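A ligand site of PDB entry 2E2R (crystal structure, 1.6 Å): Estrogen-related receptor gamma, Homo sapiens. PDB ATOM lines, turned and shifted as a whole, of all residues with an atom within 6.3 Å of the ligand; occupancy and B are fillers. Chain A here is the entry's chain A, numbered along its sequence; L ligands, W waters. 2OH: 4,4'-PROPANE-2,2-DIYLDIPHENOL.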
ATOM      1  N   LEU A  50      -4.272  22.959  18.863  1.00  0.00           N
ATOM      2  CA  LEU A  50      -4.749  22.463  20.155  1.00  0.00           C
ATOM      3  C   LEU A  50      -4.393  23.462  21.258  1.00  0.00           C
ATOM      4  O   LEU A  50      -5.172  23.678  22.177  1.00  0.00           O
ATOM      5  CB  LEU A  50      -4.155  21.074  20.454  1.00  0.00           C
ATOM      6  CG  LEU A  50      -4.649  19.990  19.501  1.00  0.00           C
ATOM      7  CD1 LEU A  50      -3.799  18.738  19.634  1.00  0.00           C
ATOM      8  CD2 LEU A  50      -6.102  19.640  19.747  1.00  0.00           C
ATOM      9  N   LEU A  53      -6.920  26.313  20.919  1.00  0.00           N
ATOM     10  CA  LEU A  53      -8.238  25.896  21.398  1.00  0.00           C
ATOM     11  C   LEU A  53      -8.301  25.795  22.911  1.00  0.00           C
ATOM     12  O   LEU A  53      -9.287  26.219  23.508  1.00  0.00           O
ATOM     13  CB  LEU A  53      -8.646  24.570  20.745  1.00  0.00           C
ATOM     14  CG  LEU A  53      -9.001  24.683  19.283  1.00  0.00           C
ATOM     15  CD1 LEU A  53      -9.061  23.254  18.736  1.00  0.00           C
ATOM     16  CD2 LEU A  53     -10.307  25.411  19.052  1.00  0.00           C
ATOM     17  N   CYS A  54      -7.278  25.223  23.542  1.00  0.00           N
ATOM     18  CA  CYS A  54      -7.277  25.080  24.998  1.00  0.00           C
ATOM     19  C   CYS A  54      -7.109  26.409  25.695  1.00  0.00           C
ATOM     20  O   CYS A  54      -7.632  26.607  26.794  1.00  0.00           O
ATOM     21  CB  CYS A  54      -6.233  24.091  25.462  1.00  0.00           C
ATOM     22  SG  CYS A  54      -6.589  22.393  24.921  1.00  0.00           S
ATOM     23  N   LEU A  56      -8.282  29.282  24.458  1.00  0.00           N
ATOM     24  CA  LEU A  56      -9.598  29.875  24.302  1.00  0.00           C
ATOM     25  C   LEU A  56     -10.536  29.294  25.357  1.00  0.00           C
ATOM     26  O   LEU A  56     -11.255  30.041  26.010  1.00  0.00           O
ATOM     27  CB  LEU A  56     -10.114  29.608  22.892  1.00  0.00           C
ATOM     28  CG  LEU A  56     -11.571  29.948  22.584  1.00  0.00           C
ATOM     29  CD1 LEU A  56     -11.845  31.421  22.690  1.00  0.00           C
ATOM     30  CD2 LEU A  56     -11.951  29.461  21.207  1.00  0.00           C
ATOM     31  N   ALA A  57     -10.521  27.985  25.534  1.00  0.00           N
ATOM     32  CA  ALA A  57     -11.383  27.320  26.532  1.00  0.00           C
ATOM     33  C   ALA A  57     -11.113  27.851  27.929  1.00  0.00           C
ATOM     34  O   ALA A  57     -12.028  28.117  28.706  1.00  0.00           O
ATOM     35  CB  ALA A  57     -11.199  25.800  26.492  1.00  0.00           C
ATOM     36  N   GLU A  60     -12.730  31.148  28.293  1.00  0.00           N
ATOM     37  CA  GLU A  60     -14.179  30.963  28.327  1.00  0.00           C
ATOM     38  C   GLU A  60     -14.624  30.440  29.679  1.00  0.00           C
ATOM     39  O   GLU A  60     -15.695  30.846  30.165  1.00  0.00           O
ATOM     40  CB  GLU A  60     -14.655  30.024  27.237  1.00  0.00           C
ATOM     41  CG  GLU A  60     -14.581  30.596  25.853  1.00  0.00           C
ATOM     42  CD  GLU A  60     -15.246  29.682  24.864  1.00  0.00           C
ATOM     43  OE1 GLU A  60     -16.479  29.665  24.866  1.00  0.00           O
ATOM     44  OE2 GLU A  60     -14.527  28.992  24.118  1.00  0.00           O
ATOM     45  N   TRP A  90     -18.778  21.616  32.430  1.00  0.00           N
ATOM     46  CA  TRP A  90     -18.020  22.616  31.662  1.00  0.00           C
ATOM     47  C   TRP A  90     -17.860  22.317  30.200  1.00  0.00           C
ATOM     48  O   TRP A  90     -17.962  23.231  29.376  1.00  0.00           O
ATOM     49  CB  TRP A  90     -16.641  22.836  32.284  1.00  0.00           C
ATOM     50  CG  TRP A  90     -15.700  21.663  32.185  1.00  0.00           C
ATOM     51  CD1 TRP A  90     -15.705  20.545  32.963  1.00  0.00           C
ATOM     52  CD2 TRP A  90     -14.611  21.500  31.270  1.00  0.00           C
ATOM     53  NE1 TRP A  90     -14.696  19.693  32.580  1.00  0.00           N
ATOM     54  CE2 TRP A  90     -14.005  20.260  31.546  1.00  0.00           C
ATOM     55  CE3 TRP A  90     -14.080  22.279  30.243  1.00  0.00           C
ATOM     56  CZ2 TRP A  90     -12.904  19.778  30.847  1.00  0.00           C
ATOM     57  CZ3 TRP A  90     -12.994  21.796  29.537  1.00  0.00           C
ATOM     58  CH2 TRP A  90     -12.421  20.564  29.844  1.00  0.00           C
ATOM     59  N   MET A  91     -17.594  21.060  29.849  1.00  0.00           N
ATOM     60  CA  MET A  91     -17.338  20.699  28.475  1.00  0.00           C
ATOM     61  C   MET A  91     -18.638  20.809  27.675  1.00  0.00           C
ATOM     62  O   MET A  91     -18.657  21.221  26.518  1.00  0.00           O
ATOM     63  CB  MET A  91     -16.746  19.297  28.397  1.00  0.00           C
ATOM     64  CG  MET A  91     -16.493  18.855  26.993  1.00  0.00           C
ATOM     65  SD  MET A  91     -15.158  19.786  26.146  1.00  0.00           S
ATOM     66  CE  MET A  91     -13.835  18.988  26.899  1.00  0.00           C
ATOM     67  N   LEU A  94     -19.144  24.493  26.947  1.00  0.00           N
ATOM     68  CA  LEU A  94     -18.232  24.929  25.891  1.00  0.00           C
ATOM     69  C   LEU A  94     -18.706  24.436  24.514  1.00  0.00           C
ATOM     70  O   LEU A  94     -18.796  25.207  23.571  1.00  0.00           O
ATOM     71  CB  LEU A  94     -16.813  24.422  26.166  1.00  0.00           C
ATOM     72  CG  LEU A  94     -16.002  25.106  27.259  1.00  0.00           C
ATOM     73  CD1 LEU A  94     -14.720  24.361  27.460  1.00  0.00           C
ATOM     74  CD2 LEU A  94     -15.762  26.605  26.943  1.00  0.00           C
ATOM     75  N   ILE A  95     -19.060  23.146  24.421  1.00  0.00           N
ATOM     76  CA  ILE A  95     -19.490  22.588  23.165  1.00  0.00           C
ATOM     77  C   ILE A  95     -20.822  23.197  22.682  1.00  0.00           C
ATOM     78  O   ILE A  95     -20.993  23.513  21.521  1.00  0.00           O
ATOM     79  CB  ILE A  95     -19.547  21.033  23.250  1.00  0.00           C
ATOM     80  CG1 ILE A  95     -18.089  20.504  23.335  1.00  0.00           C
ATOM     81  CG2 ILE A  95     -20.296  20.485  22.050  1.00  0.00           C
ATOM     82  CD1 ILE A  95     -17.957  18.960  23.563  1.00  0.00           C
ATOM     83  N   GLY A  97     -21.848  26.121  23.132  1.00  0.00           N
ATOM     84  CA  GLY A  97     -21.458  27.404  22.587  1.00  0.00           C
ATOM     85  C   GLY A  97     -20.927  27.342  21.166  1.00  0.00           C
ATOM     86  O   GLY A  97     -21.409  28.054  20.305  1.00  0.00           O
ATOM     87  N   VAL A  98     -19.952  26.466  20.878  1.00  0.00           N
ATOM     88  CA  VAL A  98     -19.459  26.379  19.503  1.00  0.00           C
ATOM     89  C   VAL A  98     -20.584  25.895  18.557  1.00  0.00           C
ATOM     90  O   VAL A  98     -20.723  26.381  17.440  1.00  0.00           O
ATOM     91  CB  VAL A  98     -18.155  25.563  19.335  1.00  0.00           C
ATOM     92  CG1 VAL A  98     -18.245  24.142  19.824  1.00  0.00           C
ATOM     93  CG2 VAL A  98     -17.693  25.587  17.865  1.00  0.00           C
ATOM     94  N   ARG A 101     -22.788  28.923  17.820  1.00  0.00           N
ATOM     95  CA  ARG A 101     -22.080  29.887  16.967  1.00  0.00           C
ATOM     96  C   ARG A 101     -21.990  29.387  15.522  1.00  0.00           C
ATOM     97  O   ARG A 101     -21.779  30.185  14.595  1.00  0.00           O
ATOM     98  CB  ARG A 101     -20.701  30.158  17.514  1.00  0.00           C
ATOM     99  CG  ARG A 101     -20.683  30.917  18.834  1.00  0.00           C
ATOM    100  CD  ARG A 101     -19.315  31.391  19.288  1.00  0.00           C
ATOM    101  NE  ARG A 101     -18.365  30.313  19.541  1.00  0.00           N
ATOM    102  CZ  ARG A 101     -18.196  29.668  20.685  1.00  0.00           C
ATOM    103  NH1 ARG A 101     -18.988  29.910  21.719  1.00  0.00           N
ATOM    104  NH2 ARG A 101     -17.256  28.746  20.803  1.00  0.00           N
ATOM    105  N   LEU A 109     -16.961  24.849  12.049  1.00  0.00           N
ATOM    106  CA  LEU A 109     -17.205  25.116  13.474  1.00  0.00           C
ATOM    107  C   LEU A 109     -16.554  26.448  13.868  1.00  0.00           C
ATOM    108  O   LEU A 109     -15.335  26.606  13.756  1.00  0.00           O
ATOM    109  CB  LEU A 109     -16.639  23.985  14.315  1.00  0.00           C
ATOM    110  CG  LEU A 109     -17.371  22.643  14.126  1.00  0.00           C
ATOM    111  CD1 LEU A 109     -16.667  21.612  14.947  1.00  0.00           C
ATOM    112  CD2 LEU A 109     -18.834  22.780  14.535  1.00  0.00           C
ATOM    113  N   VAL A 110     -17.388  27.357  14.353  1.00  0.00           N
ATOM    114  CA  VAL A 110     -16.982  28.714  14.713  1.00  0.00           C
ATOM    115  C   VAL A 110     -16.590  28.730  16.184  1.00  0.00           C
ATOM    116  O   VAL A 110     -17.391  29.113  17.054  1.00  0.00           O
ATOM    117  CB  VAL A 110     -18.105  29.721  14.432  1.00  0.00           C
ATOM    118  CG1 VAL A 110     -17.649  31.130  14.762  1.00  0.00           C
ATOM    119  CG2 VAL A 110     -18.539  29.634  12.975  1.00  0.00           C
ATOM    120  N   TYR A 111     -15.365  28.305  16.481  1.00  0.00           N
ATOM    121  CA  TYR A 111     -14.845  28.358  17.842  1.00  0.00           C
ATOM    122  C   TYR A 111     -14.766  29.811  18.312  1.00  0.00           C
ATOM    123  O   TYR A 111     -15.051  30.119  19.465  1.00  0.00           O
ATOM    124  CB  TYR A 111     -13.502  27.608  17.960  1.00  0.00           C
ATOM    125  CG  TYR A 111     -13.744  26.120  17.972  1.00  0.00           C
ATOM    126  CD1 TYR A 111     -13.729  25.363  16.792  1.00  0.00           C
ATOM    127  CD2 TYR A 111     -14.093  25.467  19.152  1.00  0.00           C
ATOM    128  CE1 TYR A 111     -14.032  23.987  16.822  1.00  0.00           C
ATOM    129  CE2 TYR A 111     -14.403  24.113  19.181  1.00  0.00           C
ATOM    130  CZ  TYR A 111     -14.371  23.376  18.020  1.00  0.00           C
ATOM    131  OH  TYR A 111     -14.704  22.033  18.100  1.00  0.00           O
ATOM    132  N   MET A 117     -13.027  26.293  12.051  1.00  0.00           N
ATOM    133  CA  MET A 117     -12.416  25.039  11.614  1.00  0.00           C
ATOM    134  C   MET A 117     -13.266  24.343  10.571  1.00  0.00           C
ATOM    135  O   MET A 117     -14.429  24.054  10.810  1.00  0.00           O
ATOM    136  CB  MET A 117     -12.169  24.104  12.774  1.00  0.00           C
ATOM    137  CG  MET A 117     -11.240  24.648  13.849  1.00  0.00           C
ATOM    138  SD  MET A 117     -10.816  23.470  15.097  1.00  0.00           S
ATOM    139  CE  MET A 117      -9.756  22.376  14.202  1.00  0.00           C
ATOM    140  N   LEU A 127      -8.757  16.064  15.432  1.00  0.00           N
ATOM    141  CA  LEU A 127     -10.094  16.247  15.957  1.00  0.00           C
ATOM    142  C   LEU A 127     -11.200  15.901  14.955  1.00  0.00           C
ATOM    143  O   LEU A 127     -12.322  16.372  15.103  1.00  0.00           O
ATOM    144  CB  LEU A 127     -10.284  17.717  16.408  1.00  0.00           C
ATOM    145  CG  LEU A 127      -9.399  18.214  17.546  1.00  0.00           C
ATOM    146  CD1 LEU A 127      -9.509  19.741  17.735  1.00  0.00           C
ATOM    147  CD2 LEU A 127      -9.714  17.493  18.828  1.00  0.00           C
ATOM    148  N   LEU A 130     -14.233  14.034  16.704  1.00  0.00           N
ATOM    149  CA  LEU A 130     -14.889  14.836  17.719  1.00  0.00           C
ATOM    150  C   LEU A 130     -15.611  16.002  17.062  1.00  0.00           C
ATOM    151  O   LEU A 130     -16.769  16.275  17.368  1.00  0.00           O
ATOM    152  CB  LEU A 130     -13.898  15.367  18.769  1.00  0.00           C
ATOM    153  CG  LEU A 130     -13.583  14.482  19.971  1.00  0.00           C
ATOM    154  CD1 LEU A 130     -12.560  15.209  20.814  1.00  0.00           C
ATOM    155  CD2 LEU A 130     -14.851  14.168  20.794  1.00  0.00           C
ATOM    156  N   ASN A 131     -14.945  16.698  16.137  1.00  0.00           N
ATOM    157  CA  ASN A 131     -15.603  17.801  15.452  1.00  0.00           C
ATOM    158  C   ASN A 131     -16.762  17.316  14.571  1.00  0.00           C
ATOM    159  O   ASN A 131     -17.756  18.014  14.405  1.00  0.00           O
ATOM    160  CB  ASN A 131     -14.604  18.644  14.661  1.00  0.00           C
ATOM    161  CG  ASN A 131     -13.865  19.669  15.530  1.00  0.00           C
ATOM    162  OD1 ASN A 131     -14.117  19.819  16.735  1.00  0.00           O
ATOM    163  ND2 ASN A 131     -12.931  20.375  14.902  1.00  0.00           N
ATOM    164  N   ILE A 134     -19.647  17.118  16.879  1.00  0.00           N
ATOM    165  CA  ILE A 134     -20.147  18.453  17.141  1.00  0.00           C
ATOM    166  C   ILE A 134     -20.982  18.925  15.936  1.00  0.00           C
ATOM    167  O   ILE A 134     -22.024  19.540  16.092  1.00  0.00           O
ATOM    168  CB  ILE A 134     -18.968  19.415  17.474  1.00  0.00           C
ATOM    169  CG1 ILE A 134     -18.285  18.946  18.770  1.00  0.00           C
ATOM    170  CG2 ILE A 134     -19.432  20.864  17.614  1.00  0.00           C
ATOM    171  CD1 ILE A 134     -17.112  19.812  19.226  1.00  0.00           C
ATOM    172  N   ALA A 216     -14.955  14.076  24.491  1.00  0.00           N
ATOM    173  CA  ALA A 216     -14.026  15.212  24.414  1.00  0.00           C
ATOM    174  C   ALA A 216     -13.165  15.336  25.677  1.00  0.00           C
ATOM    175  O   ALA A 216     -11.956  15.632  25.622  1.00  0.00           O
ATOM    176  CB  ALA A 216     -14.770  16.506  24.135  1.00  0.00           C
ATOM    177  N   PHE A 220      -9.045  15.167  25.553  1.00  0.00           N
ATOM    178  CA  PHE A 220      -8.165  16.216  26.019  1.00  0.00           C
ATOM    179  C   PHE A 220      -7.421  15.809  27.287  1.00  0.00           C
ATOM    180  O   PHE A 220      -6.322  16.311  27.545  1.00  0.00           O
ATOM    181  CB  PHE A 220      -8.913  17.545  26.142  1.00  0.00           C
ATOM    182  CG  PHE A 220      -9.084  18.217  24.825  1.00  0.00           C
ATOM    183  CD1 PHE A 220     -10.206  18.003  24.029  1.00  0.00           C
ATOM    184  CD2 PHE A 220      -8.054  19.024  24.332  1.00  0.00           C
ATOM    185  CE1 PHE A 220     -10.308  18.603  22.791  1.00  0.00           C
ATOM    186  CE2 PHE A 220      -8.165  19.622  23.098  1.00  0.00           C
ATOM    187  CZ  PHE A 220      -9.277  19.412  22.322  1.00  0.00           C
ATOM    188  N   PHE A 235      -8.323  25.410  32.962  1.00  0.00           N
ATOM    189  CA  PHE A 235      -8.636  24.319  32.027  1.00  0.00           C
ATOM    190  C   PHE A 235      -8.168  22.995  32.658  1.00  0.00           C
ATOM    191  O   PHE A 235      -8.869  21.993  32.621  1.00  0.00           O
ATOM    192  CB  PHE A 235      -7.925  24.561  30.708  1.00  0.00           C
ATOM    193  CG  PHE A 235      -8.287  23.603  29.617  1.00  0.00           C
ATOM    194  CD1 PHE A 235      -9.447  23.768  28.881  1.00  0.00           C
ATOM    195  CD2 PHE A 235      -7.432  22.565  29.282  1.00  0.00           C
ATOM    196  CE1 PHE A 235      -9.775  22.883  27.866  1.00  0.00           C
ATOM    197  CE2 PHE A 235      -7.761  21.680  28.267  1.00  0.00           C
ATOM    198  CZ  PHE A 235      -8.927  21.843  27.560  1.00  0.00           C
HETATM  199  O2  2OH L   1     -15.540  27.163  22.657  1.00  0.00           O
HETATM  200  C13 2OH L   1     -14.781  26.065  22.801  1.00  0.00           C
HETATM  201  C12 2OH L   1     -15.369  24.817  22.722  1.00  0.00           C
HETATM  202  C11 2OH L   1     -14.591  23.665  22.911  1.00  0.00           C
HETATM  203  C14 2OH L   1     -13.406  26.154  23.018  1.00  0.00           C
HETATM  204  C15 2OH L   1     -12.622  24.998  23.193  1.00  0.00           C
HETATM  205  C4  2OH L   1     -13.204  23.724  23.132  1.00  0.00           C
HETATM  206  C2  2OH L   1     -12.395  22.455  23.330  1.00  0.00           C
HETATM  207  C3  2OH L   1     -10.877  22.682  23.292  1.00  0.00           C
HETATM  208  C5  2OH L   1     -12.697  21.993  24.754  1.00  0.00           C
HETATM  209  C1  2OH L   1     -12.768  21.424  22.283  1.00  0.00           C
HETATM  210  C10 2OH L   1     -12.338  21.627  20.977  1.00  0.00           C
HETATM  211  C9  2OH L   1     -12.646  20.734  19.973  1.00  0.00           C
HETATM  212  C6  2OH L   1     -13.526  20.279  22.564  1.00  0.00           C
HETATM  213  C7  2OH L   1     -13.822  19.380  21.535  1.00  0.00           C
HETATM  214  C8  2OH L   1     -13.400  19.600  20.245  1.00  0.00           C
HETATM  215  O1  2OH L   1     -13.688  18.738  19.250  1.00  0.00           O
HETATM  216  O   HOH W   1     -18.273  28.034  23.861  1.00  0.00           O
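The side-chain amide oxygen (OD1) of Asn 131 is in hydrogen-bond range of an oxygen (O1) of the ligand (2.8 Å). The guanidinium group (NH2) of Arg 101 sits at hydrogen-bond distance from an oxygen (O2) of the ligand. O2 of the ligand sits at hydrogen-bond distance from OE2 of Glu 60 (2.6 Å).
The side-chain amide oxygen (OD1) of Asn 131 lies within hydrogen-bond range of the side-chain hydroxyl (OH) of Tyr 111, at 2.7 Å. NH1 of Arg 101 lies close to O of Gly 97. NH2 of Arg 101 is in hydrogen-bond range of O of Tyr 111, at 2.9 Å. ND2 of Asn 131 lies within hydrogen-bond range of SD of Met 117, at 3.8 Å. The guanidinium group of Arg 101 is in hydrogen-bond range of the backbone carbonyl oxygen of Val 110 (2.9 Å).
Leu 53 touches the ligand (O to C15, 3.6 Å). Ala 57 touches the ligand (CB to C15, 3.7 Å). Met 91 touches the ligand. Leu 94 touches the ligand. Tyr 111 touches the ligand (OH to C9, 3.1 Å). Leu 127 touches the ligand. Leu 130 touches the ligand (CB to O1, 3.4 Å). CD1 of Ile 134 touches O1 of the ligand (3.6 Å). CB of Ala 216 touches C7 of the ligand, 3.99 Å away. CE1 of Phe 220 touches C6 of the ligand, 3.6 Å away. Hydrophobic or aromatic side chains that line the ligand: Leu 53, Ala 57, Met 91, Leu 94, Tyr 111, Leu 127, Leu 130, Ile 134, Ala 216 and Phe 220. Along chain A the residues within 4 Å of the ligand span positions 53 to 220.
Water W1 lies within hydrogen-bond range of the side-chain carboxylate (OE1) of Glu 60 (2.6 Å), the backbone carbonyl oxygen (O) of Leu 94 (2.9 Å), the guanidinium group (NH1) of Arg 101 (2.9 Å) and an oxygen (O2) of the ligand (3.1 Å).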
